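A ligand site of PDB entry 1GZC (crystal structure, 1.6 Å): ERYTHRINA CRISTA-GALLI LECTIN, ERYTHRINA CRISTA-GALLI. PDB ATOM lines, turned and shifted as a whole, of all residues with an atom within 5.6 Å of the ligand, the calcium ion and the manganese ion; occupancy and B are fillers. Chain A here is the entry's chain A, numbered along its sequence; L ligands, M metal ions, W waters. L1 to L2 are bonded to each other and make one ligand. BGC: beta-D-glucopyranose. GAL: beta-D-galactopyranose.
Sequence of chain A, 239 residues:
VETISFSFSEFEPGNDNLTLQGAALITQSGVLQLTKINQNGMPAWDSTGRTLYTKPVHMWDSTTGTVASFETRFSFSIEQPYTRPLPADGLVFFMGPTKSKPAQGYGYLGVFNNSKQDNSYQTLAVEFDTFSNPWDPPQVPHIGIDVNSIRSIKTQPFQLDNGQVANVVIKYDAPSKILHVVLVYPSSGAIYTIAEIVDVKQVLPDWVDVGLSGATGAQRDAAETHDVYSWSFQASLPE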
ATOM      1  N   PRO A  85     -16.805  10.692 -23.837  1.00  0.00           N
ATOM      2  CA  PRO A  85     -16.021  10.977 -22.635  1.00  0.00           C
ATOM      3  C   PRO A  85     -15.609  12.454 -22.654  1.00  0.00           C
ATOM      4  O   PRO A  85     -16.168  13.252 -23.420  1.00  0.00           O
ATOM      5  CB  PRO A  85     -14.842  10.020 -22.784  1.00  0.00           C
ATOM      6  CG  PRO A  85     -14.576  10.018 -24.277  1.00  0.00           C
ATOM      7  CD  PRO A  85     -15.995  10.002 -24.866  1.00  0.00           C
ATOM      8  N   LEU A  86     -14.652  12.846 -21.818  1.00  0.00           N
ATOM      9  CA  LEU A  86     -14.215  14.252 -21.821  1.00  0.00           C
ATOM     10  C   LEU A  86     -13.471  14.539 -23.146  1.00  0.00           C
ATOM     11  O   LEU A  86     -12.786  13.670 -23.691  1.00  0.00           O
ATOM     12  CB  LEU A  86     -13.254  14.498 -20.676  1.00  0.00           C
ATOM     13  CG  LEU A  86     -13.861  14.399 -19.285  1.00  0.00           C
ATOM     14  CD1 LEU A  86     -12.805  14.653 -18.239  1.00  0.00           C
ATOM     15  CD2 LEU A  86     -14.994  15.443 -19.219  1.00  0.00           C
ATOM     16  N   ALA A  88     -10.683  16.305 -25.841  1.00  0.00           N
ATOM     17  CA  ALA A  88      -9.220  16.398 -25.790  1.00  0.00           C
ATOM     18  C   ALA A  88      -8.742  16.602 -27.227  1.00  0.00           C
ATOM     19  O   ALA A  88      -9.496  16.339 -28.149  1.00  0.00           O
ATOM     20  CB  ALA A  88      -8.647  15.063 -25.263  1.00  0.00           C
ATOM     21  N   ASP A  89      -7.521  17.085 -27.457  1.00  0.00           N
ATOM     22  CA  ASP A  89      -6.543  17.474 -26.434  1.00  0.00           C
ATOM     23  C   ASP A  89      -6.216  18.974 -26.539  1.00  0.00           C
ATOM     24  O   ASP A  89      -5.794  19.555 -25.560  1.00  0.00           O
ATOM     25  CB  ASP A  89      -5.257  16.684 -26.619  1.00  0.00           C
ATOM     26  CG  ASP A  89      -5.218  15.398 -25.762  1.00  0.00           C
ATOM     27  OD1 ASP A  89      -5.066  15.548 -24.510  1.00  0.00           O
ATOM     28  OD2 ASP A  89      -5.345  14.264 -26.337  1.00  0.00           O
ATOM     29  N   TYR A 106      -1.710  13.304 -28.529  1.00  0.00           N
ATOM     30  CA  TYR A 106      -2.512  13.409 -27.298  1.00  0.00           C
ATOM     31  C   TYR A 106      -2.139  14.687 -26.537  1.00  0.00           C
ATOM     32  O   TYR A 106      -2.098  15.766 -27.143  1.00  0.00           O
ATOM     33  CB  TYR A 106      -2.351  12.145 -26.418  1.00  0.00           C
ATOM     34  CG  TYR A 106      -2.636  10.860 -27.182  1.00  0.00           C
ATOM     35  CD1 TYR A 106      -3.652  10.795 -28.119  1.00  0.00           C
ATOM     36  CD2 TYR A 106      -1.865   9.699 -26.959  1.00  0.00           C
ATOM     37  CE1 TYR A 106      -3.916   9.598 -28.833  1.00  0.00           C
ATOM     38  CE2 TYR A 106      -2.103   8.516 -27.662  1.00  0.00           C
ATOM     39  CZ  TYR A 106      -3.124   8.480 -28.592  1.00  0.00           C
ATOM     40  OH  TYR A 106      -3.327   7.311 -29.301  1.00  0.00           O
ATOM     41  N   GLY A 107      -1.870  14.585 -25.225  1.00  0.00           N
ATOM     42  CA  GLY A 107      -1.562  15.778 -24.457  1.00  0.00           C
ATOM     43  C   GLY A 107      -0.276  16.501 -24.815  1.00  0.00           C
ATOM     44  O   GLY A 107      -0.040  17.624 -24.321  1.00  0.00           O
ATOM     45  N   GLU A 127      -0.239  27.350 -26.002  1.00  0.00           N
ATOM     46  CA  GLU A 127      -1.278  26.321 -26.164  1.00  0.00           C
ATOM     47  C   GLU A 127      -2.675  26.742 -25.735  1.00  0.00           C
ATOM     48  O   GLU A 127      -2.827  27.637 -24.892  1.00  0.00           O
ATOM     49  CB  GLU A 127      -0.855  25.117 -25.329  1.00  0.00           C
ATOM     50  CG  GLU A 127      -0.771  25.452 -23.809  1.00  0.00           C
ATOM     51  CD  GLU A 127      -0.617  24.194 -22.932  1.00  0.00           C
ATOM     52  OE1 GLU A 127       0.282  23.387 -23.223  1.00  0.00           O
ATOM     53  OE2 GLU A 127      -1.397  24.061 -21.933  1.00  0.00           O
ATOM     54  N   ASP A 129      -5.383  24.440 -24.449  1.00  0.00           N
ATOM     55  CA  ASP A 129      -5.441  23.049 -23.977  1.00  0.00           C
ATOM     56  C   ASP A 129      -6.787  22.685 -23.390  1.00  0.00           C
ATOM     57  O   ASP A 129      -7.274  23.346 -22.462  1.00  0.00           O
ATOM     58  CB  ASP A 129      -4.355  22.944 -22.897  1.00  0.00           C
ATOM     59  CG  ASP A 129      -4.091  21.518 -22.391  1.00  0.00           C
ATOM     60  OD1 ASP A 129      -4.843  20.621 -22.701  1.00  0.00           O
ATOM     61  OD2 ASP A 129      -3.064  21.323 -21.678  1.00  0.00           O
ATOM     62  N   THR A 130      -7.375  21.612 -23.922  1.00  0.00           N
ATOM     63  CA  THR A 130      -8.707  21.224 -23.528  1.00  0.00           C
ATOM     64  C   THR A 130      -8.841  20.005 -22.625  1.00  0.00           C
ATOM     65  O   THR A 130      -9.977  19.686 -22.218  1.00  0.00           O
ATOM     66  CB  THR A 130      -9.519  20.985 -24.790  1.00  0.00           C
ATOM     67  OG1 THR A 130      -8.823  19.998 -25.568  1.00  0.00           O
ATOM     68  CG2 THR A 130      -9.602  22.307 -25.637  1.00  0.00           C
ATOM     69  N   PHE A 131      -7.736  19.358 -22.271  1.00  0.00           N
ATOM     70  CA  PHE A 131      -7.802  18.171 -21.426  1.00  0.00           C
ATOM     71  C   PHE A 131      -6.795  18.302 -20.308  1.00  0.00           C
ATOM     72  O   PHE A 131      -5.628  18.593 -20.565  1.00  0.00           O
ATOM     73  CB  PHE A 131      -7.509  16.900 -22.269  1.00  0.00           C
ATOM     74  CG  PHE A 131      -7.606  15.626 -21.456  1.00  0.00           C
ATOM     75  CD1 PHE A 131      -8.841  14.954 -21.321  1.00  0.00           C
ATOM     76  CD2 PHE A 131      -6.489  15.167 -20.774  1.00  0.00           C
ATOM     77  CE1 PHE A 131      -8.937  13.810 -20.482  1.00  0.00           C
ATOM     78  CE2 PHE A 131      -6.551  14.036 -19.942  1.00  0.00           C
ATOM     79  CZ  PHE A 131      -7.790  13.364 -19.798  1.00  0.00           C
ATOM     80  N   SER A 132      -7.246  18.088 -19.058  1.00  0.00           N
ATOM     81  CA  SER A 132      -6.330  18.213 -17.928  1.00  0.00           C
ATOM     82  C   SER A 132      -5.510  16.926 -17.674  1.00  0.00           C
ATOM     83  O   SER A 132      -6.007  15.948 -17.069  1.00  0.00           O
ATOM     84  CB  SER A 132      -7.100  18.590 -16.641  1.00  0.00           C
ATOM     85  OG  SER A 132      -6.159  18.915 -15.621  1.00  0.00           O
ATOM     86  N   ASN A 133      -4.277  16.899 -18.171  1.00  0.00           N
ATOM     87  CA  ASN A 133      -3.344  15.805 -17.997  1.00  0.00           C
ATOM     88  C   ASN A 133      -2.701  15.883 -16.572  1.00  0.00           C
ATOM     89  O   ASN A 133      -2.919  16.853 -15.810  1.00  0.00           O
ATOM     90  CB  ASN A 133      -2.238  15.897 -19.071  1.00  0.00           C
ATOM     91  CG  ASN A 133      -2.769  15.686 -20.445  1.00  0.00           C
ATOM     92  OD1 ASN A 133      -3.114  16.641 -21.174  1.00  0.00           O
ATOM     93  ND2 ASN A 133      -2.883  14.413 -20.828  1.00  0.00           N
ATOM     94  N   TRP A 135       0.184  16.687 -15.637  1.00  0.00           N
ATOM     95  CA  TRP A 135       1.015  17.873 -15.473  1.00  0.00           C
ATOM     96  C   TRP A 135       0.271  19.208 -15.626  1.00  0.00           C
ATOM     97  O   TRP A 135       0.875  20.250 -15.539  1.00  0.00           O
ATOM     98  CB  TRP A 135       2.133  17.853 -16.535  1.00  0.00           C
ATOM     99  CG  TRP A 135       1.560  17.767 -17.958  1.00  0.00           C
ATOM    100  CD1 TRP A 135       1.052  18.813 -18.726  1.00  0.00           C
ATOM    101  CD2 TRP A 135       1.385  16.572 -18.741  1.00  0.00           C
ATOM    102  NE1 TRP A 135       0.570  18.313 -19.928  1.00  0.00           N
ATOM    103  CE2 TRP A 135       0.764  16.957 -19.970  1.00  0.00           C
ATOM    104  CE3 TRP A 135       1.687  15.222 -18.532  1.00  0.00           C
ATOM    105  CZ2 TRP A 135       0.457  16.028 -20.964  1.00  0.00           C
ATOM    106  CZ3 TRP A 135       1.369  14.300 -19.521  1.00  0.00           C
ATOM    107  CH2 TRP A 135       0.758  14.714 -20.735  1.00  0.00           C
ATOM    108  N   ASP A 136      -1.025  19.163 -15.832  1.00  0.00           N
ATOM    109  CA  ASP A 136      -1.824  20.379 -16.094  1.00  0.00           C
ATOM    110  C   ASP A 136      -2.582  20.914 -14.888  1.00  0.00           C
ATOM    111  O   ASP A 136      -2.809  20.188 -13.924  1.00  0.00           O
ATOM    112  CB  ASP A 136      -2.955  20.035 -17.093  1.00  0.00           C
ATOM    113  CG  ASP A 136      -2.519  20.062 -18.550  1.00  0.00           C
ATOM    114  OD1 ASP A 136      -1.751  20.966 -18.899  1.00  0.00           O
ATOM    115  OD2 ASP A 136      -2.976  19.202 -19.331  1.00  0.00           O
ATOM    116  N   PRO A 137      -2.997  22.202 -14.958  1.00  0.00           N
ATOM    117  CA  PRO A 137      -3.805  22.774 -13.878  1.00  0.00           C
ATOM    118  C   PRO A 137      -5.155  22.087 -14.175  1.00  0.00           C
ATOM    119  O   PRO A 137      -5.368  21.556 -15.268  1.00  0.00           O
ATOM    120  CB  PRO A 137      -3.835  24.278 -14.221  1.00  0.00           C
ATOM    121  CG  PRO A 137      -3.622  24.279 -15.784  1.00  0.00           C
ATOM    122  CD  PRO A 137      -2.542  23.225 -15.919  1.00  0.00           C
ATOM    123  N   HIS A 142      -7.568  25.940 -20.982  1.00  0.00           N
ATOM    124  CA  HIS A 142      -6.675  26.960 -20.479  1.00  0.00           C
ATOM    125  C   HIS A 142      -5.676  27.385 -21.557  1.00  0.00           C
ATOM    126  O   HIS A 142      -5.296  26.601 -22.419  1.00  0.00           O
ATOM    127  CB  HIS A 142      -5.872  26.520 -19.205  1.00  0.00           C
ATOM    128  CG  HIS A 142      -5.088  25.226 -19.335  1.00  0.00           C
ATOM    129  ND1 HIS A 142      -5.569  23.998 -18.919  1.00  0.00           N
ATOM    130  CD2 HIS A 142      -3.844  25.002 -19.815  1.00  0.00           C
ATOM    131  CE1 HIS A 142      -4.650  23.067 -19.149  1.00  0.00           C
ATOM    132  NE2 HIS A 142      -3.592  23.647 -19.697  1.00  0.00           N
ATOM    133  N   ILE A 150       5.915  20.795 -22.050  1.00  0.00           N
ATOM    134  CA  ILE A 150       4.448  20.786 -22.129  1.00  0.00           C
ATOM    135  C   ILE A 150       3.885  21.245 -20.737  1.00  0.00           C
ATOM    136  O   ILE A 150       2.694  21.548 -20.635  1.00  0.00           O
ATOM    137  CB  ILE A 150       3.932  19.361 -22.485  1.00  0.00           C
ATOM    138  CG1 ILE A 150       2.446  19.380 -22.819  1.00  0.00           C
ATOM    139  CG2 ILE A 150       4.080  18.428 -21.230  1.00  0.00           C
ATOM    140  CD1 ILE A 150       2.106  20.228 -24.095  1.00  0.00           C
ATOM    141  N   SER A 152       3.353  23.979 -18.647  1.00  0.00           N
ATOM    142  CA  SER A 152       3.428  25.435 -18.814  1.00  0.00           C
ATOM    143  C   SER A 152       4.010  26.174 -17.634  1.00  0.00           C
ATOM    144  O   SER A 152       3.727  25.833 -16.485  1.00  0.00           O
ATOM    145  CB  SER A 152       2.028  26.034 -19.040  1.00  0.00           C
ATOM    146  OG  SER A 152       1.285  25.327 -20.033  1.00  0.00           O
ATOM    147  N   THR A 155      -0.383  29.585 -16.840  1.00  0.00           N
ATOM    148  CA  THR A 155      -1.631  29.301 -17.532  1.00  0.00           C
ATOM    149  C   THR A 155      -2.731  30.278 -17.136  1.00  0.00           C
ATOM    150  O   THR A 155      -2.660  30.956 -16.097  1.00  0.00           O
ATOM    151  CB  THR A 155      -2.141  27.882 -17.242  1.00  0.00           C
ATOM    152  OG1 THR A 155      -2.361  27.712 -15.805  1.00  0.00           O
ATOM    153  CG2 THR A 155      -1.111  26.882 -17.703  1.00  0.00           C
ATOM    154  N   THR A 216      -6.276  15.254 -31.143  1.00  0.00           N
ATOM    155  CA  THR A 216      -7.457  14.697 -30.434  1.00  0.00           C
ATOM    156  C   THR A 216      -6.948  13.521 -29.582  1.00  0.00           C
ATOM    157  O   THR A 216      -5.799  13.141 -29.676  1.00  0.00           O
ATOM    158  CB  THR A 216      -8.600  14.266 -31.356  1.00  0.00           C
ATOM    159  OG1 THR A 216      -8.099  13.381 -32.355  1.00  0.00           O
ATOM    160  CG2 THR A 216      -9.180  15.516 -32.014  1.00  0.00           C
ATOM    161  N   GLY A 217      -7.851  12.990 -28.752  1.00  0.00           N
ATOM    162  CA  GLY A 217      -7.449  12.051 -27.719  1.00  0.00           C
ATOM    163  C   GLY A 217      -7.202  10.601 -27.930  1.00  0.00           C
ATOM    164  O   GLY A 217      -7.387  10.104 -29.034  1.00  0.00           O
ATOM    165  N   ALA A 218      -6.830   9.941 -26.828  1.00  0.00           N
ATOM    166  CA  ALA A 218      -6.419   8.530 -26.830  1.00  0.00           C
ATOM    167  C   ALA A 218      -7.504   7.470 -26.646  1.00  0.00           C
ATOM    168  O   ALA A 218      -7.158   6.286 -26.503  1.00  0.00           O
ATOM    169  CB  ALA A 218      -5.293   8.315 -25.813  1.00  0.00           C
ATOM    170  N   GLN A 219      -8.773   7.861 -26.631  1.00  0.00           N
ATOM    171  CA  GLN A 219      -9.850   6.881 -26.536  1.00  0.00           C
ATOM    172  C   GLN A 219     -11.030   7.362 -27.349  1.00  0.00           C
ATOM    173  O   GLN A 219     -11.167   8.553 -27.603  1.00  0.00           O
ATOM    174  CB  GLN A 219     -10.270   6.628 -25.069  1.00  0.00           C
ATOM    175  CG  GLN A 219     -10.900   7.809 -24.371  1.00  0.00           C
ATOM    176  CD  GLN A 219     -11.411   7.440 -22.974  1.00  0.00           C
ATOM    177  OE1 GLN A 219     -12.588   7.109 -22.808  1.00  0.00           O
ATOM    178  NE2 GLN A 219     -10.544   7.494 -21.985  1.00  0.00           N
ATOM    179  N   ALA A 222     -12.970  10.952 -27.434  1.00  0.00           N
ATOM    180  CA  ALA A 222     -12.280  12.004 -26.608  1.00  0.00           C
ATOM    181  C   ALA A 222     -11.716  12.867 -27.774  1.00  0.00           C
ATOM    182  O   ALA A 222     -10.525  12.754 -28.164  1.00  0.00           O
ATOM    183  CB  ALA A 222     -11.109  11.397 -25.770  1.00  0.00           C
HETATM  184  C2  BGC L   1      -7.083   5.646 -21.592  1.00  0.00           C
HETATM  185  C3  BGC L   1      -6.501   6.816 -22.434  1.00  0.00           C
HETATM  186  C4  BGC L   1      -5.535   7.655 -21.585  1.00  0.00           C
HETATM  187  C5  BGC L   1      -4.421   6.789 -20.960  1.00  0.00           C
HETATM  188  C6  BGC L   1      -3.571   7.594 -19.966  1.00  0.00           C
HETATM  189  C1  BGC L   1      -5.910   4.831 -21.063  1.00  0.00           C
HETATM  190  O1  BGC L   1      -6.398   3.770 -20.294  1.00  0.00           O
HETATM  191  O2  BGC L   1      -7.936   4.884 -22.435  1.00  0.00           O
HETATM  192  O3  BGC L   1      -7.583   7.596 -22.939  1.00  0.00           O
HETATM  193  O4  BGC L   1      -4.836   8.692 -22.386  1.00  0.00           O
HETATM  194  O5  BGC L   1      -5.078   5.692 -20.214  1.00  0.00           O
HETATM  195  O6  BGC L   1      -2.506   6.800 -19.457  1.00  0.00           O
HETATM  196  C1  GAL L   2      -5.310  10.046 -22.267  1.00  0.00           C
HETATM  197  C2  GAL L   2      -4.301  11.005 -22.892  1.00  0.00           C
HETATM  198  C3  GAL L   2      -4.908  12.460 -22.764  1.00  0.00           C
HETATM  199  C4  GAL L   2      -6.270  12.481 -23.472  1.00  0.00           C
HETATM  200  C5  GAL L   2      -7.192  11.429 -22.844  1.00  0.00           C
HETATM  201  C6  GAL L   2      -8.539  11.336 -23.550  1.00  0.00           C
HETATM  202  O2  GAL L   2      -3.024  10.926 -22.232  1.00  0.00           O
HETATM  203  O3  GAL L   2      -3.999  13.402 -23.326  1.00  0.00           O
HETATM  204  O4  GAL L   2      -6.178  12.145 -24.852  1.00  0.00           O
HETATM  205  O5  GAL L   2      -6.581  10.118 -22.923  1.00  0.00           O
HETATM  206  O6  GAL L   2      -9.409  10.565 -22.713  1.00  0.00           O
HETATM  207 CA    CA M   1      -3.516  18.900 -21.604  1.00  0.00          CA
HETATM  208 MN    MN M   2      -1.740  22.506 -20.445  1.00  0.00          MN
HETATM  209  O   HOH W   1      -4.314  17.968 -23.654  1.00  0.00           O
HETATM  210  O   HOH W   2      -2.524  11.646 -19.680  1.00  0.00           O
HETATM  211  O   HOH W   3      -0.037  21.457 -21.459  1.00  0.00           O
HETATM  212  O   HOH W   4      -8.897   9.878 -19.966  1.00  0.00           O
HETATM  213  O   HOH W   5      -0.451  23.571 -19.034  1.00  0.00           O
HETATM  214  O   HOH W   6      -1.228  19.022 -22.381  1.00  0.00           O
HETATM  215  O   HOH W   7     -11.603  11.564 -22.409  1.00  0.00           O
HETATM  216  O   HOH W   8      -0.970  12.699 -23.291  1.00  0.00           O
HETATM  217  O   HOH W   9      -1.710   8.747 -23.125  1.00  0.00           O
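Merely in contact with the ligand: Gly 217, Ala 222, Tyr 106 and Ala 88.
Hydrophobic or aromatic side chains within 4 Å of the ligand: Ala 88, Tyr 106, Phe 131, Ala 218 and Ala 222.
The manganese ion is bound by the side-chain carboxylate of Asp 129 (2.2 Å), the side-chain carboxylate of Glu 127 (2.2 Å), the side-chain carboxylate of Asp 136 (2.2 Å), water W5 (2.2 Å), water W3 (2.2 Å) and a ring nitrogen (NE2) of His 142 (2.3 Å).
The manganese ion has six donor atoms within binding distance.
Water W6 bridges the backbone carbonyl oxygen of Gly 107 (2.7 Å) and the indole nitrogen of Trp 135 (3.1 Å).
Water W3 lies within hydrogen-bond range of the side-chain carboxylate of Glu 127 and the backbone carbonyl oxygen of Ile 150.
Water W7 bridges an oxygen (O6) of GAL L2 (2.4 Å) and the backbone carbonyl oxygen (O) of Leu 86 (2.7 Å).
Water W2 bridges an oxygen (O2) of GAL L2 and the side-chain amide nitrogen of Asn 133.
Water W8 lies within hydrogen-bond range of the backbone NH of Gly 107 (2.8 Å) and an oxygen (O2) of GAL L2 (2.9 Å).
Four residues have an atom within 4 Å of the calcium ion: Asp 129, Phe 131, Asn 133 and Asp 136.
The nearest printed residue that does not touch the calcium ion is Trp 135 (4.5 Å).
The calcium ion is bound by OD1 of Asn 133 (2.3 Å), OD2 of Asp 136 (2.4 Å), O of Phe 131 (2.4 Å), water W1 (2.4 Å), water W6 (2.4 Å), OD1 of Asp 129 (2.4 Å) and OD2 of Asp 129 (2.5 Å).
The backbone NH (N) of Gly 107 lies within hydrogen-bond range of the side-chain carboxylate (OD1) of Asp 89 (3.4 Å).
The side-chain hydroxyl (OG1) of Thr 130 lies close to the backbone carbonyl oxygen (O) of Asp 89 (3.1 Å).
N of Gly 217 is in hydrogen-bond range of O of Ala 222 (2.7 Å).
Along chain A the residues within 4 Å of the manganese ion span positions 127 to 142.
The nearest printed residue that does not touch the manganese ion is Ser 152 (4.2 Å).
The side-chain amide nitrogen (ND2) of Asn 133 lies within hydrogen-bond range of an oxygen (O3) of GAL L2, at 2.9 Å.
The side-chain carboxylate of Asp 89 is in hydrogen-bond range of an oxygen (O3) of GAL L2 (2.7 Å).
The backbone NH (N) of Ala 218 sits at hydrogen-bond distance from an oxygen (O4) of GAL L2 (3.0 Å).
N of Gly 107 sits at hydrogen-bond distance from O3 of GAL L2, 3.1 Å away.
O3 of BGC L1 sits at hydrogen-bond distance from NE2 of Gln 219 (3.1 Å).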
